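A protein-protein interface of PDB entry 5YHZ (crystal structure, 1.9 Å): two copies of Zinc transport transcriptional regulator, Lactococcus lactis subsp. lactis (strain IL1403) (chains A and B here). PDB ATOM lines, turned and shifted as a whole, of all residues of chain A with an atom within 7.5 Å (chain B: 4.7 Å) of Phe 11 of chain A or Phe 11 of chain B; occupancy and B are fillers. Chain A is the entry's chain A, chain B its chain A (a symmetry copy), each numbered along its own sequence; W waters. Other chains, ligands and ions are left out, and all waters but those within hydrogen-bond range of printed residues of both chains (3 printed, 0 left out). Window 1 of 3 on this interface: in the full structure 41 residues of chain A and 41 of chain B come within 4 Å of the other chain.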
ATOM      1  N   MET A   2     -14.180 -31.269  14.374  1.00  0.00           N
ATOM      2  CA  MET A   2     -15.589 -30.926  14.255  1.00  0.00           C
ATOM      3  C   MET A   2     -15.748 -29.430  14.043  1.00  0.00           C
ATOM      4  O   MET A   2     -14.778 -28.662  14.121  1.00  0.00           O
ATOM      5  CB  MET A   2     -16.358 -31.387  15.487  1.00  0.00           C
ATOM      6  CG  MET A   2     -15.996 -30.639  16.721  1.00  0.00           C
ATOM      7  SD  MET A   2     -16.306 -31.578  18.186  1.00  0.00           S
ATOM      8  CE  MET A   2     -14.869 -32.651  18.239  1.00  0.00           C
ATOM      9  N   LEU A   4     -16.789 -25.646  15.028  1.00  0.00           N
ATOM     10  CA  LEU A   4     -16.632 -24.975  16.273  1.00  0.00           C
ATOM     11  C   LEU A   4     -17.917 -25.132  17.077  1.00  0.00           C
ATOM     12  O   LEU A   4     -17.881 -25.276  18.299  1.00  0.00           O
ATOM     13  CB  LEU A   4     -16.306 -23.524  15.980  1.00  0.00           C
ATOM     14  CG  LEU A   4     -15.697 -22.756  17.106  1.00  0.00           C
ATOM     15  CD1 LEU A   4     -14.399 -23.385  17.546  1.00  0.00           C
ATOM     16  CD2 LEU A   4     -15.402 -21.377  16.599  1.00  0.00           C
ATOM     17  N   ALA A   5     -19.064 -25.153  16.410  1.00  0.00           N
ATOM     18  CA  ALA A   5     -20.337 -25.209  17.148  1.00  0.00           C
ATOM     19  C   ALA A   5     -20.372 -26.490  17.857  1.00  0.00           C
ATOM     20  O   ALA A   5     -20.766 -26.557  19.013  1.00  0.00           O
ATOM     21  CB  ALA A   5     -21.486 -25.153  16.253  1.00  0.00           C
ATOM     22  N   ASN A   6     -19.970 -27.541  17.169  1.00  0.00           N
ATOM     23  CA  ASN A   6     -19.913 -28.833  17.827  1.00  0.00           C
ATOM     24  C   ASN A   6     -18.874 -28.877  18.920  1.00  0.00           C
ATOM     25  O   ASN A   6     -19.072 -29.479  19.975  1.00  0.00           O
ATOM     26  CB  ASN A   6     -19.716 -29.946  16.797  1.00  0.00           C
ATOM     27  CG  ASN A   6     -20.995 -30.242  16.080  1.00  0.00           C
ATOM     28  OD1 ASN A   6     -22.066 -30.122  16.688  1.00  0.00           O
ATOM     29  ND2 ASN A   6     -20.917 -30.518  14.787  1.00  0.00           N
ATOM     30  N   GLN A   7     -17.759 -28.195  18.720  1.00  0.00           N
ATOM     31  CA  GLN A   7     -16.765 -28.271  19.774  1.00  0.00           C
ATOM     32  C   GLN A   7     -17.280 -27.498  20.973  1.00  0.00           C
ATOM     33  O   GLN A   7     -17.076 -27.874  22.076  1.00  0.00           O
ATOM     34  CB  GLN A   7     -15.443 -27.653  19.318  1.00  0.00           C
ATOM     35  CG  GLN A   7     -14.378 -27.790  20.362  1.00  0.00           C
ATOM     36  CD  GLN A   7     -12.988 -27.324  19.836  1.00  0.00           C
ATOM     37  OE1 GLN A   7     -12.866 -26.813  18.701  1.00  0.00           O
ATOM     38  NE2 GLN A   7     -11.942 -27.588  20.633  1.00  0.00           N
ATOM     39  N   ILE A   8     -17.950 -26.383  20.735  1.00  0.00           N
ATOM     40  CA  ILE A   8     -18.496 -25.641  21.850  1.00  0.00           C
ATOM     41  C   ILE A   8     -19.531 -26.499  22.547  1.00  0.00           C
ATOM     42  O   ILE A   8     -19.596 -26.600  23.767  1.00  0.00           O
ATOM     43  CB  ILE A   8     -19.215 -24.340  21.347  1.00  0.00           C
ATOM     44  CG1 ILE A   8     -18.162 -23.330  20.820  1.00  0.00           C
ATOM     45  CG2 ILE A   8     -19.949 -23.748  22.531  1.00  0.00           C
ATOM     46  CD1 ILE A   8     -18.719 -22.288  19.843  1.00  0.00           C
ATOM     47  N   ASP A   9     -20.384 -27.113  21.750  1.00  0.00           N
ATOM     48  CA  ASP A   9     -21.355 -28.040  22.377  1.00  0.00           C
ATOM     49  C   ASP A   9     -20.651 -29.123  23.254  1.00  0.00           C
ATOM     50  O   ASP A   9     -20.954 -29.282  24.464  1.00  0.00           O
ATOM     51  CB  ASP A   9     -22.232 -28.629  21.271  1.00  0.00           C
ATOM     52  CG  ASP A   9     -23.404 -29.470  21.837  1.00  0.00           C
ATOM     53  OD1 ASP A   9     -23.872 -29.221  22.942  1.00  0.00           O
ATOM     54  OD2 ASP A   9     -23.803 -30.408  21.165  1.00  0.00           O
ATOM     55  N   GLN A  10     -19.655 -29.819  22.700  1.00  0.00           N
ATOM     56  CA  GLN A  10     -18.960 -30.845  23.471  1.00  0.00           C
ATOM     57  C   GLN A  10     -18.332 -30.242  24.721  1.00  0.00           C
ATOM     58  O   GLN A  10     -18.317 -30.869  25.779  1.00  0.00           O
ATOM     59  CB  GLN A  10     -17.836 -31.517  22.682  1.00  0.00           C
ATOM     60  CG  GLN A  10     -18.365 -32.287  21.442  1.00  0.00           C
ATOM     61  CD  GLN A  10     -19.436 -33.310  21.804  1.00  0.00           C
ATOM     62  OE1 GLN A  10     -20.637 -33.067  21.603  1.00  0.00           O
ATOM     63  NE2 GLN A  10     -19.003 -34.465  22.373  1.00  0.00           N
ATOM     64  N   PHE A  11     -17.740 -29.055  24.575  1.00  0.00           N
ATOM     65  CA  PHE A  11     -17.106 -28.432  25.715  1.00  0.00           C
ATOM     66  C   PHE A  11     -18.135 -28.199  26.805  1.00  0.00           C
ATOM     67  O   PHE A  11     -17.969 -28.526  27.977  1.00  0.00           O
ATOM     68  CB  PHE A  11     -16.507 -27.088  25.283  1.00  0.00           C
ATOM     69  CG  PHE A  11     -16.150 -26.229  26.431  1.00  0.00           C
ATOM     70  CD1 PHE A  11     -15.175 -26.599  27.302  1.00  0.00           C
ATOM     71  CD2 PHE A  11     -16.774 -25.024  26.608  1.00  0.00           C
ATOM     72  CE1 PHE A  11     -14.861 -25.789  28.402  1.00  0.00           C
ATOM     73  CE2 PHE A  11     -16.437 -24.192  27.635  1.00  0.00           C
ATOM     74  CZ  PHE A  11     -15.486 -24.595  28.561  1.00  0.00           C
ATOM     75  N   LEU A  12     -19.230 -27.568  26.442  1.00  0.00           N
ATOM     76  CA  LEU A  12     -20.240 -27.318  27.496  1.00  0.00           C
ATOM     77  C   LEU A  12     -20.801 -28.639  28.063  1.00  0.00           C
ATOM     78  O   LEU A  12     -21.170 -28.720  29.259  1.00  0.00           O
ATOM     79  CB  LEU A  12     -21.383 -26.492  26.931  1.00  0.00           C
ATOM     80  CG  LEU A  12     -20.915 -25.067  26.567  1.00  0.00           C
ATOM     81  CD1 LEU A  12     -22.002 -24.337  25.818  1.00  0.00           C
ATOM     82  CD2 LEU A  12     -20.480 -24.312  27.859  1.00  0.00           C
ATOM     83  N   GLY A  13     -20.879 -29.666  27.219  1.00  0.00           N
ATOM     84  CA  GLY A  13     -21.355 -30.972  27.666  1.00  0.00           C
ATOM     85  C   GLY A  13     -20.368 -31.543  28.678  1.00  0.00           C
ATOM     86  O   GLY A  13     -20.738 -32.222  29.658  1.00  0.00           O
ATOM     87  N   THR A  14     -19.086 -31.246  28.461  1.00  0.00           N
ATOM     88  CA  THR A  14     -18.054 -31.839  29.308  1.00  0.00           C
ATOM     89  C   THR A  14     -18.123 -31.124  30.659  1.00  0.00           C
ATOM     90  O   THR A  14     -17.891 -31.720  31.697  1.00  0.00           O
ATOM     91  CB  THR A  14     -16.688 -31.611  28.709  1.00  0.00           C
ATOM     92  OG1 THR A  14     -16.617 -32.251  27.401  1.00  0.00           O
ATOM     93  CG2 THR A  14     -15.651 -32.100  29.683  1.00  0.00           C
ATOM     94  N   ILE A  15     -18.447 -29.829  30.634  1.00  0.00           N
ATOM     95  CA  ILE A  15     -18.584 -29.042  31.858  1.00  0.00           C
ATOM     96  C   ILE A  15     -19.749 -29.628  32.701  1.00  0.00           C
ATOM     97  O   ILE A  15     -19.617 -29.862  33.887  1.00  0.00           O
ATOM     98  CB  ILE A  15     -18.893 -27.528  31.519  1.00  0.00           C
ATOM     99  CG1 ILE A  15     -17.678 -26.842  30.850  1.00  0.00           C
ATOM    100  CG2 ILE A  15     -19.287 -26.779  32.800  1.00  0.00           C
ATOM    101  CD1 ILE A  15     -16.416 -26.992  31.668  1.00  0.00           C
ATOM    102  N   MET A  16     -20.903 -29.829  32.070  1.00  0.00           N
ATOM    103  CA  MET A  16     -22.091 -30.395  32.760  1.00  0.00           C
ATOM    104  C   MET A  16     -21.812 -31.803  33.291  1.00  0.00           C
ATOM    105  O   MET A  16     -22.185 -32.133  34.414  1.00  0.00           O
ATOM    106  CB  MET A  16     -23.245 -30.424  31.773  1.00  0.00           C
ATOM    107  CG  MET A  16     -23.629 -28.990  31.362  1.00  0.00           C
ATOM    108  SD  MET A  16     -23.686 -27.813  32.778  1.00  0.00           S
ATOM    109  CE  MET A  16     -25.044 -28.716  33.505  1.00  0.00           C
ATOM    110  N   GLN A  17     -21.140 -32.634  32.500  1.00  0.00           N
ATOM    111  CA  GLN A  17     -20.648 -33.942  32.981  1.00  0.00           C
ATOM    112  C   GLN A  17     -19.734 -33.753  34.191  1.00  0.00           C
ATOM    113  O   GLN A  17     -19.850 -34.430  35.205  1.00  0.00           O
ATOM    114  CB  GLN A  17     -19.869 -34.616  31.850  1.00  0.00           C
ATOM    115  CG  GLN A  17     -19.894 -36.135  31.773  1.00  0.00           C
ATOM    116  CD  GLN A  17     -19.827 -36.638  30.316  1.00  0.00           C
ATOM    117  OE1 GLN A  17     -19.632 -35.853  29.385  1.00  0.00           O
ATOM    118  NE2 GLN A  17     -20.023 -37.946  30.122  1.00  0.00           N
ATOM    119  N   ILE A  25     -17.864 -24.939  39.313  1.00  0.00           N
ATOM    120  CA  ILE A  25     -16.861 -25.705  38.614  1.00  0.00           C
ATOM    121  C   ILE A  25     -15.553 -25.515  39.329  1.00  0.00           C
ATOM    122  O   ILE A  25     -14.995 -24.429  39.369  1.00  0.00           O
ATOM    123  CB  ILE A  25     -16.712 -25.297  37.133  1.00  0.00           C
ATOM    124  CG1 ILE A  25     -18.064 -25.295  36.432  1.00  0.00           C
ATOM    125  CG2 ILE A  25     -15.721 -26.272  36.446  1.00  0.00           C
ATOM    126  CD1 ILE A  25     -18.693 -26.674  36.422  1.00  0.00           C
ATOM    127  N   PHE A 137     -14.715 -14.098  22.557  1.00  0.00           N
ATOM    128  CA  PHE A 137     -15.577 -15.296  22.323  1.00  0.00           C
ATOM    129  C   PHE A 137     -16.314 -15.586  23.595  1.00  0.00           C
ATOM    130  O   PHE A 137     -17.530 -15.797  23.662  1.00  0.00           O
ATOM    131  CB  PHE A 137     -14.636 -16.470  21.923  1.00  0.00           C
ATOM    132  CG  PHE A 137     -15.294 -17.811  22.044  1.00  0.00           C
ATOM    133  CD1 PHE A 137     -16.186 -18.216  21.098  1.00  0.00           C
ATOM    134  CD2 PHE A 137     -15.095 -18.626  23.175  1.00  0.00           C
ATOM    135  CE1 PHE A 137     -16.867 -19.467  21.236  1.00  0.00           C
ATOM    136  CE2 PHE A 137     -15.772 -19.885  23.289  1.00  0.00           C
ATOM    137  CZ  PHE A 137     -16.645 -20.255  22.304  1.00  0.00           C
ATOM    138  N   LEU A 138     -15.571 -15.598  24.684  1.00  0.00           N
ATOM    139  CA  LEU A 138     -16.201 -15.877  25.985  1.00  0.00           C
ATOM    140  C   LEU A 138     -17.336 -14.859  26.307  1.00  0.00           C
ATOM    141  O   LEU A 138     -18.351 -15.248  26.858  1.00  0.00           O
ATOM    142  CB  LEU A 138     -15.155 -15.823  27.051  1.00  0.00           C
ATOM    143  CG  LEU A 138     -14.194 -17.039  27.001  1.00  0.00           C
ATOM    144  CD1 LEU A 138     -13.190 -16.874  28.196  1.00  0.00           C
ATOM    145  CD2 LEU A 138     -14.911 -18.331  27.094  1.00  0.00           C
ATOM    146  N   SER A 139     -17.076 -13.579  26.040  1.00  0.00           N
ATOM    147  CA  SER A 139     -18.080 -12.543  26.290  1.00  0.00           C
ATOM    148  C   SER A 139     -19.333 -12.801  25.499  1.00  0.00           C
ATOM    149  O   SER A 139     -20.406 -12.769  26.024  1.00  0.00           O
ATOM    150  CB  SER A 139     -17.535 -11.176  25.927  1.00  0.00           C
ATOM    151  OG  SER A 139     -16.482 -10.895  26.842  1.00  0.00           O
ATOM    152  N   ALA A 140     -19.177 -13.058  24.219  1.00  0.00           N
ATOM    153  CA  ALA A 140     -20.307 -13.331  23.347  1.00  0.00           C
ATOM    154  C   ALA A 140     -21.026 -14.538  23.827  1.00  0.00           C
ATOM    155  O   ALA A 140     -22.234 -14.567  23.934  1.00  0.00           O
ATOM    156  CB  ALA A 140     -19.804 -13.542  21.845  1.00  0.00           C
ATOM    157  N   LEU A 141     -20.289 -15.537  24.277  1.00  0.00           N
ATOM    158  CA  LEU A 141     -20.931 -16.745  24.618  1.00  0.00           C
ATOM    159  C   LEU A 141     -21.629 -16.563  25.976  1.00  0.00           C
ATOM    160  O   LEU A 141     -22.742 -17.034  26.220  1.00  0.00           O
ATOM    161  CB  LEU A 141     -19.841 -17.893  24.649  1.00  0.00           C
ATOM    162  CG  LEU A 141     -20.506 -19.262  24.632  1.00  0.00           C
ATOM    163  CD1 LEU A 141     -21.533 -19.313  23.466  1.00  0.00           C
ATOM    164  CD2 LEU A 141     -19.434 -20.463  24.601  1.00  0.00           C
ATOM    165  N   THR A 142     -21.012 -15.741  26.817  1.00  0.00           N
ATOM    166  CA  THR A 142     -21.535 -15.578  28.148  1.00  0.00           C
ATOM    167  C   THR A 142     -22.886 -14.867  27.979  1.00  0.00           C
ATOM    168  O   THR A 142     -23.866 -15.183  28.625  1.00  0.00           O
ATOM    169  CB  THR A 142     -20.605 -14.680  28.999  1.00  0.00           C
ATOM    170  OG1 THR A 142     -19.391 -15.389  29.288  1.00  0.00           O
ATOM    171  CG2 THR A 142     -21.318 -14.261  30.334  1.00  0.00           C
ATOM    172  N   GLU A 143     -22.921 -13.936  27.053  1.00  0.00           N
ATOM    173  CA  GLU A 143     -24.153 -13.161  26.822  1.00  0.00           C
ATOM    174  C   GLU A 143     -25.315 -14.082  26.454  1.00  0.00           C
ATOM    175  O   GLU A 143     -26.484 -13.746  26.750  1.00  0.00           O
ATOM    176  CB  GLU A 143     -23.933 -12.159  25.684  1.00  0.00           C
ATOM    177  CG  GLU A 143     -22.961 -11.058  26.016  1.00  0.00           C
ATOM    178  CD  GLU A 143     -22.871 -10.016  24.895  1.00  0.00           C
ATOM    179  OE1 GLU A 143     -23.858  -9.918  24.141  1.00  0.00           O
ATOM    180  OE2 GLU A 143     -21.831  -9.313  24.787  1.00  0.00           O
ATOM    181  N   PHE A 145     -25.924 -16.898  27.594  1.00  0.00           N
ATOM    182  CA  PHE A 145     -26.369 -17.600  28.776  1.00  0.00           C
ATOM    183  C   PHE A 145     -26.873 -16.754  29.944  1.00  0.00           C
ATOM    184  O   PHE A 145     -27.034 -17.274  31.050  1.00  0.00           O
ATOM    185  CB  PHE A 145     -25.254 -18.580  29.211  1.00  0.00           C
ATOM    186  CG  PHE A 145     -24.999 -19.618  28.172  1.00  0.00           C
ATOM    187  CD1 PHE A 145     -26.020 -20.519  27.846  1.00  0.00           C
ATOM    188  CD2 PHE A 145     -23.819 -19.684  27.499  1.00  0.00           C
ATOM    189  CE1 PHE A 145     -25.813 -21.440  26.853  1.00  0.00           C
ATOM    190  CE2 PHE A 145     -23.626 -20.628  26.513  1.00  0.00           C
ATOM    191  CZ  PHE A 145     -24.620 -21.474  26.183  1.00  0.00           C
ATOM    192  N   GLN B   7     -12.213 -14.225  33.672  1.00  0.00           N
ATOM    193  CA  GLN B   7     -13.323 -14.231  32.737  1.00  0.00           C
ATOM    194  C   GLN B   7     -13.747 -15.669  32.508  1.00  0.00           C
ATOM    195  O   GLN B   7     -14.887 -15.956  32.371  1.00  0.00           O
ATOM    196  CB  GLN B   7     -12.908 -13.618  31.400  1.00  0.00           C
ATOM    197  CG  GLN B   7     -14.059 -13.542  30.445  1.00  0.00           C
ATOM    198  CD  GLN B   7     -13.686 -12.759  29.150  1.00  0.00           C
ATOM    199  OE1 GLN B   7     -12.519 -12.357  28.953  1.00  0.00           O
ATOM    200  NE2 GLN B   7     -14.704 -12.476  28.325  1.00  0.00           N
ATOM    201  N   ILE B   8     -12.793 -16.582  32.452  1.00  0.00           N
ATOM    202  CA  ILE B   8     -13.159 -17.971  32.279  1.00  0.00           C
ATOM    203  C   ILE B   8     -13.963 -18.415  33.482  1.00  0.00           C
ATOM    204  O   ILE B   8     -14.986 -19.085  33.386  1.00  0.00           O
ATOM    205  CB  ILE B   8     -11.878 -18.873  32.202  1.00  0.00           C
ATOM    206  CG1 ILE B   8     -11.130 -18.607  30.869  1.00  0.00           C
ATOM    207  CG2 ILE B   8     -12.341 -20.314  32.254  1.00  0.00           C
ATOM    208  CD1 ILE B   8      -9.646 -18.993  30.889  1.00  0.00           C
ATOM    209  N   ASP B   9     -13.473 -18.058  34.654  1.00  0.00           N
ATOM    210  CA  ASP B   9     -14.273 -18.386  35.856  1.00  0.00           C
ATOM    211  C   ASP B   9     -15.732 -17.839  35.758  1.00  0.00           C
ATOM    212  O   ASP B   9     -16.726 -18.598  35.887  1.00  0.00           O
ATOM    213  CB  ASP B   9     -13.514 -17.881  37.085  1.00  0.00           C
ATOM    214  CG  ASP B   9     -14.174 -18.338  38.411  1.00  0.00           C
ATOM    215  OD1 ASP B   9     -14.823 -19.377  38.457  1.00  0.00           O
ATOM    216  OD2 ASP B   9     -14.063 -17.603  39.379  1.00  0.00           O
ATOM    217  N   GLN B  10     -15.890 -16.549  35.448  1.00  0.00           N
ATOM    218  CA  GLN B  10     -17.230 -15.979  35.342  1.00  0.00           C
ATOM    219  C   GLN B  10     -18.043 -16.713  34.282  1.00  0.00           C
ATOM    220  O   GLN B  10     -19.242 -16.925  34.448  1.00  0.00           O
ATOM    221  CB  GLN B  10     -17.215 -14.501  34.955  1.00  0.00           C
ATOM    222  CG  GLN B  10     -16.526 -13.617  36.029  1.00  0.00           C
ATOM    223  CD  GLN B  10     -17.144 -13.791  37.412  1.00  0.00           C
ATOM    224  OE1 GLN B  10     -16.582 -14.487  38.274  1.00  0.00           O
ATOM    225  NE2 GLN B  10     -18.335 -13.173  37.625  1.00  0.00           N
ATOM    226  N   PHE B  11     -17.400 -17.026  33.154  1.00  0.00           N
ATOM    227  CA  PHE B  11     -18.114 -17.705  32.097  1.00  0.00           C
ATOM    228  C   PHE B  11     -18.635 -19.036  32.607  1.00  0.00           C
ATOM    229  O   PHE B  11     -19.794 -19.412  32.461  1.00  0.00           O
ATOM    230  CB  PHE B  11     -17.158 -17.947  30.923  1.00  0.00           C
ATOM    231  CG  PHE B  11     -17.686 -18.927  29.951  1.00  0.00           C
ATOM    232  CD1 PHE B  11     -18.807 -18.661  29.231  1.00  0.00           C
ATOM    233  CD2 PHE B  11     -17.026 -20.107  29.737  1.00  0.00           C
ATOM    234  CE1 PHE B  11     -19.314 -19.608  28.330  1.00  0.00           C
ATOM    235  CE2 PHE B  11     -17.468 -21.014  28.818  1.00  0.00           C
ATOM    236  CZ  PHE B  11     -18.644 -20.771  28.126  1.00  0.00           C
ATOM    237  N   LEU B  12     -17.752 -19.818  33.189  1.00  0.00           N
ATOM    238  CA  LEU B  12     -18.238 -21.127  33.681  1.00  0.00           C
ATOM    239  C   LEU B  12     -19.299 -20.955  34.788  1.00  0.00           C
ATOM    240  O   LEU B  12     -20.224 -21.791  34.928  1.00  0.00           O
ATOM    241  CB  LEU B  12     -17.075 -21.939  34.225  1.00  0.00           C
ATOM    242  CG  LEU B  12     -16.101 -22.342  33.099  1.00  0.00           C
ATOM    243  CD1 LEU B  12     -14.855 -22.960  33.684  1.00  0.00           C
ATOM    244  CD2 LEU B  12     -16.819 -23.298  32.100  1.00  0.00           C
ATOM    245  N   GLY B  13     -19.170 -19.892  35.578  1.00  0.00           N
ATOM    246  CA  GLY B  13     -20.144 -19.613  36.630  1.00  0.00           C
ATOM    247  C   GLY B  13     -21.491 -19.297  35.990  1.00  0.00           C
ATOM    248  O   GLY B  13     -22.572 -19.646  36.508  1.00  0.00           O
ATOM    249  N   THR B  14     -21.437 -18.648  34.827  1.00  0.00           N
ATOM    250  CA  THR B  14     -22.673 -18.200  34.191  1.00  0.00           C
ATOM    251  C   THR B  14     -23.351 -19.443  33.610  1.00  0.00           C
ATOM    252  O   THR B  14     -24.565 -19.543  33.586  1.00  0.00           O
ATOM    253  CB  THR B  14     -22.368 -17.244  33.064  1.00  0.00           C
ATOM    254  OG1 THR B  14     -21.685 -16.070  33.593  1.00  0.00           O
ATOM    255  CG2 THR B  14     -23.651 -16.929  32.344  1.00  0.00           C
ATOM    256  N   ILE B  15     -22.544 -20.396  33.137  1.00  0.00           N
ATOM    257  CA  ILE B  15     -23.064 -21.649  32.592  1.00  0.00           C
ATOM    258  C   ILE B  15     -23.808 -22.414  33.719  1.00  0.00           C
ATOM    259  O   ILE B  15     -24.919 -22.874  33.546  1.00  0.00           O
ATOM    260  CB  ILE B  15     -21.888 -22.549  32.035  1.00  0.00           C
ATOM    261  CG1 ILE B  15     -21.240 -21.915  30.780  1.00  0.00           C
ATOM    262  CG2 ILE B  15     -22.418 -23.952  31.708  1.00  0.00           C
ATOM    263  CD1 ILE B  15     -22.260 -21.594  29.712  1.00  0.00           C
ATOM    264  N   LEU B 138     -10.545 -24.090  23.726  1.00  0.00           N
ATOM    265  CA  LEU B 138     -11.606 -25.009  24.171  1.00  0.00           C
ATOM    266  C   LEU B 138     -11.052 -26.438  24.449  1.00  0.00           C
ATOM    267  O   LEU B 138     -11.486 -27.075  25.393  1.00  0.00           O
ATOM    268  CB  LEU B 138     -12.665 -25.072  23.118  1.00  0.00           C
ATOM    269  CG  LEU B 138     -13.509 -23.772  23.046  1.00  0.00           C
ATOM    270  CD1 LEU B 138     -14.600 -24.000  21.943  1.00  0.00           C
ATOM    271  CD2 LEU B 138     -14.137 -23.434  24.343  1.00  0.00           C
ATOM    272  N   LEU B 141      -9.141 -26.498  27.554  1.00  0.00           N
ATOM    273  CA  LEU B 141      -9.939 -26.311  28.701  1.00  0.00           C
ATOM    274  C   LEU B 141     -10.776 -27.579  28.928  1.00  0.00           C
ATOM    275  O   LEU B 141     -10.985 -28.046  30.050  1.00  0.00           O
ATOM    276  CB  LEU B 141     -10.838 -25.028  28.473  1.00  0.00           C
ATOM    277  CG  LEU B 141     -11.432 -24.550  29.790  1.00  0.00           C
ATOM    278  CD1 LEU B 141     -10.295 -24.422  30.843  1.00  0.00           C
ATOM    279  CD2 LEU B 141     -12.307 -23.210  29.618  1.00  0.00           C
ATOM    280  N   THR B 142     -11.136 -28.219  27.821  1.00  0.00           N
ATOM    281  CA  THR B 142     -12.000 -29.366  27.924  1.00  0.00           C
ATOM    282  C   THR B 142     -11.173 -30.448  28.634  1.00  0.00           C
ATOM    283  O   THR B 142     -11.650 -31.164  29.492  1.00  0.00           O
ATOM    284  CB  THR B 142     -12.395 -29.884  26.520  1.00  0.00           C
ATOM    285  OG1 THR B 142     -13.287 -28.947  25.898  1.00  0.00           O
ATOM    286  CG2 THR B 142     -13.079 -31.294  26.628  1.00  0.00           C
ATOM    287  N   PHE B 145     -11.312 -30.667  32.299  1.00  0.00           N
ATOM    288  CA  PHE B 145     -12.551 -31.158  32.857  1.00  0.00           C
ATOM    289  C   PHE B 145     -12.912 -32.617  32.582  1.00  0.00           C
ATOM    290  O   PHE B 145     -14.053 -33.019  32.820  1.00  0.00           O
ATOM    291  CB  PHE B 145     -13.687 -30.194  32.444  1.00  0.00           C
ATOM    292  CG  PHE B 145     -13.482 -28.829  33.007  1.00  0.00           C
ATOM    293  CD1 PHE B 145     -13.491 -28.657  34.396  1.00  0.00           C
ATOM    294  CD2 PHE B 145     -13.238 -27.755  32.209  1.00  0.00           C
ATOM    295  CE1 PHE B 145     -13.246 -27.416  34.923  1.00  0.00           C
ATOM    296  CE2 PHE B 145     -13.009 -26.511  32.759  1.00  0.00           C
ATOM    297  CZ  PHE B 145     -12.990 -26.356  34.096  1.00  0.00           C
HETATM  298  O   HOH W   1     -14.406 -22.444  37.435  1.00  0.00           O
HETATM  299  O   HOH W   2     -17.423 -13.513  29.834  1.00  0.00           O
HETATM  300  O   HOH W   3     -13.127 -29.317  23.154  1.00  0.00           O
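OG of Ser 139 of chain A sits at hydrogen-bond distance from NE2 of Gln 7 of chain B (2.8 Å).
The backbone carbonyl oxygen (O) of Leu 138 of chain B is in hydrogen-bond range of the side-chain hydroxyl (OG1) of Thr 142 of chain B (2.6 Å).
O of Leu 138 of chain A is in hydrogen-bond range of OG1 of Thr 142 of chain A.
O of Gln 10 of chain B sits at hydrogen-bond distance from OG1 of Thr 14 of chain B (2.7 Å).
The side-chain hydroxyl (OG1) of Thr 14 of chain A lies within hydrogen-bond range of the backbone carbonyl oxygen (O) of Gln 10 of chain A, 2.7 Å away.
SD of Met 2 of chain A sits close to N of Gln 7 of chain A.
Among the printed residues, merely in contact across the chains: Gln 7 of chain A with Leu 138 of chain B (3.6 Å), Ile 8 of chain A with Leu 138 of chain B (3.8 Å), Phe 11 of chain A with Phe 11 of chain B (3.5 Å), Phe 11 of chain A with Leu 12 of chain B (3.998 Å), Phe 11 of chain A with Leu 138 of chain B (3.8 Å), Phe 11 of chain A with Leu 141 of chain B (3.6 Å), Phe 11 of chain A with Thr 142 of chain B (3.3 Å), Leu 12 of chain A with Phe 11 of chain B (3.998 Å), Leu 12 of chain A with Ile 15 of chain B (3.7 Å), Thr 14 of chain A with Thr 142 of chain B (3.7 Å), Thr 14 of chain A with Phe 145 of chain B (3.6 Å), Ile 15 of chain A with Leu 12 of chain B (3.7 Å), Ile 15 of chain A with Phe 145 of chain B (3.3 Å), Ile 25 of chain A with Phe 145 of chain B (3.1 Å), Leu 138 of chain A with Gln 7 of chain B (3.6 Å), Leu 138 of chain A with Ile 8 of chain B (3.8 Å), Leu 138 of chain A with Phe 11 of chain B (3.8 Å), Leu 141 of chain A with Phe 11 of chain B (3.6 Å), Thr 142 of chain A with Phe 11 of chain B (3.3 Å), Thr 142 of chain A with Thr 14 of chain B (3.7 Å), Phe 145 of chain A with Thr 14 of chain B (3.6 Å) and Phe 145 of chain A with Ile 15 of chain B (3.3 Å).
Of the printed residues of chain A, Phe 11 of chain B touches Phe 11, Leu 12, Leu 138, Leu 141 and Thr 142.
Of the printed residues of chain A, Ile 15 of chain B touches Leu 12 (3.7 Å) and Phe 145 (3.3 Å).
Printed residues of chain A within 4 Å of Thr 14 of chain B: Thr 142 (3.7 Å) and Phe 145 (3.6 Å).
Printed residues of chain A within 4 Å of Gln 7 of chain B: Leu 138 (3.6 Å) and Ser 139 (2.8 Å).
Of the printed residues of chain B, Leu 141 of chain A touches Phe 11.
Met 2 of chain A touches none of the printed residues of chain B.
Gln 10 of chain B touches none of the printed residues of chain A.
Hydrophobic or aromatic side chains of chain A within 4 Å of the printed part of chain B: Ile 8, Phe 11, Leu 12, Ile 15, Ile 25, Leu 138, Leu 141 and Phe 145.
Among the printed residues, 23 pairs touch across the chains.
Phe 11 of chain A touches Leu 138 of chain B, and with the chains exchanged Leu 138 of chain A touches Phe 11 of chain B.
Leu 12 of chain A touches Ile 15 of chain B, and with the chains exchanged Ile 15 of chain A touches Leu 12 of chain B.
Thr 14 of chain A touches Thr 142 of chain B, and with the chains exchanged Thr 142 of chain A touches Thr 14 of chain B.
Of the 23 pairs that touch across the chains among the printed residues, 21 have their exchanged pair printed and touching as well.
Water W2 lies within hydrogen-bond range of the side-chain hydroxyl (OG1) of Thr 142 of chain A and the side-chain amide nitrogen (NE2) of Gln 7 of chain B.
Water W3 lies within hydrogen-bond range of the side-chain hydroxyl of Thr 142 of chain B (2.8 Å) and the side-chain amide nitrogen of Gln 7 of chain A (3.3 Å).
Water W1 lies within hydrogen-bond range of O of Ile 25 of chain A (2.8 Å) and OD1 of Asp 9 of chain B (3.3 Å).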
